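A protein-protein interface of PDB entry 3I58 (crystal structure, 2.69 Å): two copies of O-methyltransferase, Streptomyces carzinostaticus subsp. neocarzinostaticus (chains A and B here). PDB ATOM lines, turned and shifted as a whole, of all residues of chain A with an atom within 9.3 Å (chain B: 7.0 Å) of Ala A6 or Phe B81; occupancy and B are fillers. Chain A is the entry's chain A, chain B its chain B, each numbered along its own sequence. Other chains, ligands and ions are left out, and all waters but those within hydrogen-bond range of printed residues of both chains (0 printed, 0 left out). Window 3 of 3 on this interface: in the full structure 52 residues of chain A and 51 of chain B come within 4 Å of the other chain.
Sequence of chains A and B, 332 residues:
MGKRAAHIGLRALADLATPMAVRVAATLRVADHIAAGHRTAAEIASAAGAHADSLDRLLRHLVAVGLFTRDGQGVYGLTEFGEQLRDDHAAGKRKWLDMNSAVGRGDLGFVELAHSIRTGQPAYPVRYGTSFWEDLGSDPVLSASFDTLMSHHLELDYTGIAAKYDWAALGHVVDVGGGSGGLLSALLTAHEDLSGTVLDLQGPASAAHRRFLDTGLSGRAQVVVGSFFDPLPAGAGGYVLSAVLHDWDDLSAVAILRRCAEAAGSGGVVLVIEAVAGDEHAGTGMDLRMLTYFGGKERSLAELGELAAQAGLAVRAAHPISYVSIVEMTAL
The backbone carbonyl oxygen (O) of Leu B67 lies close to the backbone NH (N) of Thr B79, at 3.4 Å. OG1 of Thr B79 lies close to N of Phe B81.
Among the printed residues, pairs that only touch across the chains: Ala A5 with Ala B64 (3.5 Å), Ala A6 with Phe B81 (3.6 Å), Leu A10 with Gln B84 (3.99 Å), Leu A10 with Leu B85 (3.99 Å), Leu A13 with Val B65 (3.9 Å) and Leu A13 with Leu B67 (3.96 Å).
No position is printed for both chains.
The backbone carbonyl oxygen of Val B65 sits close to the backbone NH of Ala A5, at 3.4 Å. The backbone NH (N) of Ala A6 is in hydrogen-bond range of the backbone carbonyl oxygen (O) of Val B65.
Of the 14 printed residues of chain B, 6 touch a printed residue of chain A. Hydrophobic or aromatic side chains of chain B within 4 Å of the printed part of chain A: Val B65, Leu B67, Phe B81 and Leu B85. Among the printed residues, 8 pairs touch across the chains. Among the printed residues, no Asp or Glu carboxylate lies within 4 Å of a Lys or Arg side-chain nitrogen of the other chain.
Of chain B, only Val B65 (3.2 Å) and Phe B81 (3.6 Å) come within 4 Å of Ala A6. Printed residues of chain A within 4 Å of Phe B81: Ala A6. No residue of chain A comes within 4 Å of Gly B66. Glu B80 touches none of the printed residues of chain A. No residue of chain A comes within 4 Å of Gly B82. Of the printed residues of chain A, Leu B67 touches Leu A13. Of the printed residues of chain B, Leu A13 touches Val B65 (3.9 Å) and Leu B67 (3.96 Å). Of the printed residues of chain A, Leu B85 touches Leu A10. The nearest residue of chain B that does not touch Ala A6 is Gly B66 (4.2 Å). The nearest residue of chain A that does not touch Phe B81 is Leu A10 (5.2 Å). The nearest printed residue of chain B that does not touch Leu A13 is Gly B66 (6.4 Å).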
ATOM      1  N   ALA A   5       9.488   2.901   2.366  1.00  0.00           N
ATOM      2  CA  ALA A   5       9.435   1.424   2.177  1.00  0.00           C
ATOM      3  C   ALA A   5       8.093   0.826   2.622  1.00  0.00           C
ATOM      4  O   ALA A   5       7.648   1.014   3.761  1.00  0.00           O
ATOM      5  CB  ALA A   5      10.583   0.760   2.935  1.00  0.00           C
ATOM      6  N   ALA A   6       7.454   0.114   1.693  1.00  0.00           N
ATOM      7  CA  ALA A   6       6.171  -0.547   1.930  1.00  0.00           C
ATOM      8  C   ALA A   6       6.379  -2.066   1.965  1.00  0.00           C
ATOM      9  O   ALA A   6       6.451  -2.732   0.921  1.00  0.00           O
ATOM     10  CB  ALA A   6       5.170  -0.178   0.829  1.00  0.00           C
ATOM     11  N   HIS A   7       6.499  -2.593   3.179  1.00  0.00           N
ATOM     12  CA  HIS A   7       6.676  -4.021   3.405  1.00  0.00           C
ATOM     13  C   HIS A   7       5.414  -4.423   4.161  1.00  0.00           C
ATOM     14  O   HIS A   7       5.441  -5.265   5.062  1.00  0.00           O
ATOM     15  CB  HIS A   7       7.907  -4.261   4.267  1.00  0.00           C
ATOM     16  CG  HIS A   7       7.899  -3.486   5.549  1.00  0.00           C
ATOM     17  ND1 HIS A   7       6.929  -3.658   6.515  1.00  0.00           N
ATOM     18  CD2 HIS A   7       8.727  -2.521   6.015  1.00  0.00           C
ATOM     19  CE1 HIS A   7       7.161  -2.832   7.521  1.00  0.00           C
ATOM     20  NE2 HIS A   7       8.246  -2.132   7.243  1.00  0.00           N
ATOM     21  N   ILE A   8       4.313  -3.778   3.781  1.00  0.00           N
ATOM     22  CA  ILE A   8       2.999  -4.000   4.374  1.00  0.00           C
ATOM     23  C   ILE A   8       1.915  -3.849   3.295  1.00  0.00           C
ATOM     24  O   ILE A   8       1.969  -2.932   2.471  1.00  0.00           O
ATOM     25  CB  ILE A   8       2.769  -3.005   5.538  1.00  0.00           C
ATOM     26  CG1 ILE A   8       1.338  -2.477   5.516  1.00  0.00           C
ATOM     27  CG2 ILE A   8       3.778  -1.866   5.452  1.00  0.00           C
ATOM     28  CD1 ILE A   8       1.059  -1.461   6.600  1.00  0.00           C
ATOM     29  N   GLY A   9       0.945  -4.765   3.313  1.00  0.00           N
ATOM     30  CA  GLY A   9      -0.139  -4.781   2.339  1.00  0.00           C
ATOM     31  C   GLY A   9      -0.862  -3.546   1.830  1.00  0.00           C
ATOM     32  O   GLY A   9      -1.380  -2.753   2.613  1.00  0.00           O
ATOM     33  N   LEU A  10      -0.907  -3.393   0.508  1.00  0.00           N
ATOM     34  CA  LEU A  10      -1.574  -2.254  -0.115  1.00  0.00           C
ATOM     35  C   LEU A  10      -2.873  -1.825   0.558  1.00  0.00           C
ATOM     36  O   LEU A  10      -3.064  -0.656   0.868  1.00  0.00           O
ATOM     37  CB  LEU A  10      -1.831  -2.520  -1.605  1.00  0.00           C
ATOM     38  CG  LEU A  10      -2.018  -1.386  -2.634  1.00  0.00           C
ATOM     39  CD1 LEU A  10      -3.409  -1.445  -3.226  1.00  0.00           C
ATOM     40  CD2 LEU A  10      -1.746  -0.036  -2.005  1.00  0.00           C
ATOM     41  N   ARG A  11      -3.766  -2.777   0.793  1.00  0.00           N
ATOM     42  CA  ARG A  11      -5.037  -2.442   1.414  1.00  0.00           C
ATOM     43  C   ARG A  11      -4.828  -1.974   2.851  1.00  0.00           C
ATOM     44  O   ARG A  11      -5.510  -1.059   3.323  1.00  0.00           O
ATOM     45  CB  ARG A  11      -5.993  -3.645   1.358  1.00  0.00           C
ATOM     46  CG  ARG A  11      -7.349  -3.295   0.748  1.00  0.00           C
ATOM     47  CD  ARG A  11      -7.783  -4.276  -0.333  1.00  0.00           C
ATOM     48  NE  ARG A  11      -8.697  -5.314   0.150  1.00  0.00           N
ATOM     49  CZ  ARG A  11      -9.879  -5.079   0.721  1.00  0.00           C
ATOM     50  NH1 ARG A  11     -10.306  -3.833   0.894  1.00  0.00           N
ATOM     51  NH2 ARG A  11     -10.646  -6.096   1.109  1.00  0.00           N
ATOM     52  N   ALA A  12      -3.870  -2.589   3.537  1.00  0.00           N
ATOM     53  CA  ALA A  12      -3.575  -2.219   4.912  1.00  0.00           C
ATOM     54  C   ALA A  12      -2.917  -0.845   4.924  1.00  0.00           C
ATOM     55  O   ALA A  12      -3.045  -0.077   5.874  1.00  0.00           O
ATOM     56  CB  ALA A  12      -2.653  -3.232   5.523  1.00  0.00           C
ATOM     57  N   LEU A  13      -2.204  -0.543   3.854  1.00  0.00           N
ATOM     58  CA  LEU A  13      -1.522   0.728   3.727  1.00  0.00           C
ATOM     59  C   LEU A  13      -2.578   1.840   3.584  1.00  0.00           C
ATOM     60  O   LEU A  13      -2.331   3.004   3.912  1.00  0.00           O
ATOM     61  CB  LEU A  13      -0.610   0.656   2.503  1.00  0.00           C
ATOM     62  CG  LEU A  13       0.514   1.652   2.253  1.00  0.00           C
ATOM     63  CD1 LEU A  13       1.464   1.688   3.429  1.00  0.00           C
ATOM     64  CD2 LEU A  13       1.248   1.232   0.988  1.00  0.00           C
ATOM     65  N   ALA B  64       7.791   8.023  -1.597  1.00  0.00           N
ATOM     66  CA  ALA B  64       8.349   7.954  -0.255  1.00  0.00           C
ATOM     67  C   ALA B  64       7.770   6.751   0.487  1.00  0.00           C
ATOM     68  O   ALA B  64       8.464   6.087   1.258  1.00  0.00           O
ATOM     69  CB  ALA B  64       8.026   9.224   0.498  1.00  0.00           C
ATOM     70  N   VAL B  65       6.490   6.478   0.255  1.00  0.00           N
ATOM     71  CA  VAL B  65       5.830   5.359   0.915  1.00  0.00           C
ATOM     72  C   VAL B  65       6.352   4.039   0.377  1.00  0.00           C
ATOM     73  O   VAL B  65       6.357   3.025   1.082  1.00  0.00           O
ATOM     74  CB  VAL B  65       4.317   5.389   0.695  1.00  0.00           C
ATOM     75  CG1 VAL B  65       3.675   4.272   1.496  1.00  0.00           C
ATOM     76  CG2 VAL B  65       3.759   6.742   1.090  1.00  0.00           C
ATOM     77  N   GLY B  66       6.771   4.056  -0.883  1.00  0.00           N
ATOM     78  CA  GLY B  66       7.295   2.853  -1.498  1.00  0.00           C
ATOM     79  C   GLY B  66       6.433   2.263  -2.599  1.00  0.00           C
ATOM     80  O   GLY B  66       6.543   1.074  -2.898  1.00  0.00           O
ATOM     81  N   LEU B  67       5.583   3.072  -3.218  1.00  0.00           N
ATOM     82  CA  LEU B  67       4.732   2.553  -4.275  1.00  0.00           C
ATOM     83  C   LEU B  67       5.226   2.961  -5.647  1.00  0.00           C
ATOM     84  O   LEU B  67       5.011   2.255  -6.625  1.00  0.00           O
ATOM     85  CB  LEU B  67       3.288   3.031  -4.089  1.00  0.00           C
ATOM     86  CG  LEU B  67       2.555   2.565  -2.829  1.00  0.00           C
ATOM     87  CD1 LEU B  67       1.114   3.065  -2.866  1.00  0.00           C
ATOM     88  CD2 LEU B  67       2.595   1.047  -2.731  1.00  0.00           C
ATOM     89  N   PHE B  68       5.885   4.106  -5.722  1.00  0.00           N
ATOM     90  CA  PHE B  68       6.387   4.585  -6.997  1.00  0.00           C
ATOM     91  C   PHE B  68       7.868   4.924  -6.903  1.00  0.00           C
ATOM     92  O   PHE B  68       8.463   4.878  -5.830  1.00  0.00           O
ATOM     93  CB  PHE B  68       5.605   5.828  -7.464  1.00  0.00           C
ATOM     94  CG  PHE B  68       4.114   5.618  -7.575  1.00  0.00           C
ATOM     95  CD1 PHE B  68       3.592   4.473  -8.165  1.00  0.00           C
ATOM     96  CD2 PHE B  68       3.228   6.581  -7.105  1.00  0.00           C
ATOM     97  CE1 PHE B  68       2.202   4.291  -8.283  1.00  0.00           C
ATOM     98  CE2 PHE B  68       1.839   6.406  -7.221  1.00  0.00           C
ATOM     99  CZ  PHE B  68       1.329   5.259  -7.811  1.00  0.00           C
ATOM    100  N   LEU B  78       6.452   2.400 -11.443  1.00  0.00           N
ATOM    101  CA  LEU B  78       5.889   1.596 -10.369  1.00  0.00           C
ATOM    102  C   LEU B  78       6.989   0.820  -9.659  1.00  0.00           C
ATOM    103  O   LEU B  78       8.156   0.931 -10.016  1.00  0.00           O
ATOM    104  CB  LEU B  78       4.847   0.629 -10.933  1.00  0.00           C
ATOM    105  CG  LEU B  78       3.476   1.223 -11.276  1.00  0.00           C
ATOM    106  CD1 LEU B  78       3.633   2.592 -11.903  1.00  0.00           C
ATOM    107  CD2 LEU B  78       2.734   0.286 -12.213  1.00  0.00           C
ATOM    108  N   THR B  79       6.620   0.047  -8.643  1.00  0.00           N
ATOM    109  CA  THR B  79       7.590  -0.755  -7.906  1.00  0.00           C
ATOM    110  C   THR B  79       6.982  -2.124  -7.656  1.00  0.00           C
ATOM    111  O   THR B  79       5.808  -2.351  -7.955  1.00  0.00           O
ATOM    112  CB  THR B  79       7.962  -0.128  -6.536  1.00  0.00           C
ATOM    113  OG1 THR B  79       6.977  -0.477  -5.556  1.00  0.00           O
ATOM    114  CG2 THR B  79       8.060   1.388  -6.649  1.00  0.00           C
ATOM    115  N   GLU B  80       7.779  -3.030  -7.105  1.00  0.00           N
ATOM    116  CA  GLU B  80       7.322  -4.384  -6.828  1.00  0.00           C
ATOM    117  C   GLU B  80       5.992  -4.350  -6.073  1.00  0.00           C
ATOM    118  O   GLU B  80       5.152  -5.248  -6.209  1.00  0.00           O
ATOM    119  CB  GLU B  80       8.377  -5.117  -5.997  1.00  0.00           C
ATOM    120  CG  GLU B  80       8.275  -6.633  -6.031  1.00  0.00           C
ATOM    121  CD  GLU B  80       8.032  -7.242  -4.657  1.00  0.00           C
ATOM    122  OE1 GLU B  80       6.850  -7.328  -4.238  1.00  0.00           O
ATOM    123  OE2 GLU B  80       9.025  -7.626  -3.993  1.00  0.00           O
ATOM    124  N   PHE B  81       5.801  -3.291  -5.292  1.00  0.00           N
ATOM    125  CA  PHE B  81       4.596  -3.140  -4.484  1.00  0.00           C
ATOM    126  C   PHE B  81       3.547  -2.267  -5.159  1.00  0.00           C
ATOM    127  O   PHE B  81       2.355  -2.565  -5.103  1.00  0.00           O
ATOM    128  CB  PHE B  81       4.994  -2.570  -3.127  1.00  0.00           C
ATOM    129  CG  PHE B  81       6.285  -3.139  -2.614  1.00  0.00           C
ATOM    130  CD1 PHE B  81       6.377  -4.492  -2.271  1.00  0.00           C
ATOM    131  CD2 PHE B  81       7.428  -2.344  -2.524  1.00  0.00           C
ATOM    132  CE1 PHE B  81       7.588  -5.047  -1.850  1.00  0.00           C
ATOM    133  CE2 PHE B  81       8.646  -2.890  -2.103  1.00  0.00           C
ATOM    134  CZ  PHE B  81       8.722  -4.246  -1.766  1.00  0.00           C
ATOM    135  N   GLY B  82       3.995  -1.199  -5.809  1.00  0.00           N
ATOM    136  CA  GLY B  82       3.069  -0.305  -6.481  1.00  0.00           C
ATOM    137  C   GLY B  82       2.380  -0.957  -7.662  1.00  0.00           C
ATOM    138  O   GLY B  82       1.466  -0.386  -8.263  1.00  0.00           O
ATOM    139  N   GLU B  83       2.825  -2.162  -7.990  1.00  0.00           N
ATOM    140  CA  GLU B  83       2.271  -2.904  -9.109  1.00  0.00           C
ATOM    141  C   GLU B  83       0.826  -3.289  -8.808  1.00  0.00           C
ATOM    142  O   GLU B  83      -0.009  -3.363  -9.719  1.00  0.00           O
ATOM    143  CB  GLU B  83       3.110  -4.161  -9.351  1.00  0.00           C
ATOM    144  CG  GLU B  83       3.226  -4.583 -10.812  1.00  0.00           C
ATOM    145  CD  GLU B  83       4.010  -3.584 -11.649  1.00  0.00           C
ATOM    146  OE1 GLU B  83       5.038  -3.074 -11.149  1.00  0.00           O
ATOM    147  OE2 GLU B  83       3.609  -3.315 -12.808  1.00  0.00           O
ATOM    148  N   GLN B  84       0.539  -3.519  -7.525  1.00  0.00           N
ATOM    149  CA  GLN B  84      -0.797  -3.903  -7.081  1.00  0.00           C
ATOM    150  C   GLN B  84      -1.838  -2.799  -7.215  1.00  0.00           C
ATOM    151  O   GLN B  84      -3.001  -3.009  -6.869  1.00  0.00           O
ATOM    152  CB  GLN B  84      -0.773  -4.343  -5.624  1.00  0.00           C
ATOM    153  CG  GLN B  84       0.222  -5.416  -5.296  1.00  0.00           C
ATOM    154  CD  GLN B  84       0.110  -5.850  -3.847  1.00  0.00           C
ATOM    155  OE1 GLN B  84      -0.843  -6.530  -3.466  1.00  0.00           O
ATOM    156  NE2 GLN B  84       1.073  -5.439  -3.025  1.00  0.00           N
ATOM    157  N   LEU B  85      -1.436  -1.626  -7.694  1.00  0.00           N
ATOM    158  CA  LEU B  85      -2.381  -0.529  -7.848  1.00  0.00           C
ATOM    159  C   LEU B  85      -3.016  -0.522  -9.223  1.00  0.00           C
ATOM    160  O   LEU B  85      -4.028   0.145  -9.451  1.00  0.00           O
ATOM    161  CB  LEU B  85      -1.700   0.815  -7.582  1.00  0.00           C
ATOM    162  CG  LEU B  85      -1.811   1.298  -6.131  1.00  0.00           C
ATOM    163  CD1 LEU B  85      -0.938   2.536  -5.915  1.00  0.00           C
ATOM    164  CD2 LEU B  85      -3.278   1.588  -5.819  1.00  0.00           C
ATOM    165  N   HIS B  89      -3.921  -5.988 -12.263  1.00  0.00           N
ATOM    166  CA  HIS B  89      -3.213  -6.835 -11.305  1.00  0.00           C
ATOM    167  C   HIS B  89      -4.093  -7.988 -10.818  1.00  0.00           C
ATOM    168  O   HIS B  89      -5.308  -7.852 -10.672  1.00  0.00           O
ATOM    169  CB  HIS B  89      -2.749  -6.011 -10.108  1.00  0.00           C
ATOM    170  CG  HIS B  89      -1.916  -6.781  -9.132  1.00  0.00           C
ATOM    171  ND1 HIS B  89      -0.561  -6.974  -9.298  1.00  0.00           N
ATOM    172  CD2 HIS B  89      -2.250  -7.424  -7.988  1.00  0.00           C
ATOM    173  CE1 HIS B  89      -0.096  -7.703  -8.297  1.00  0.00           C
ATOM    174  NE2 HIS B  89      -1.102  -7.989  -7.488  1.00  0.00           N
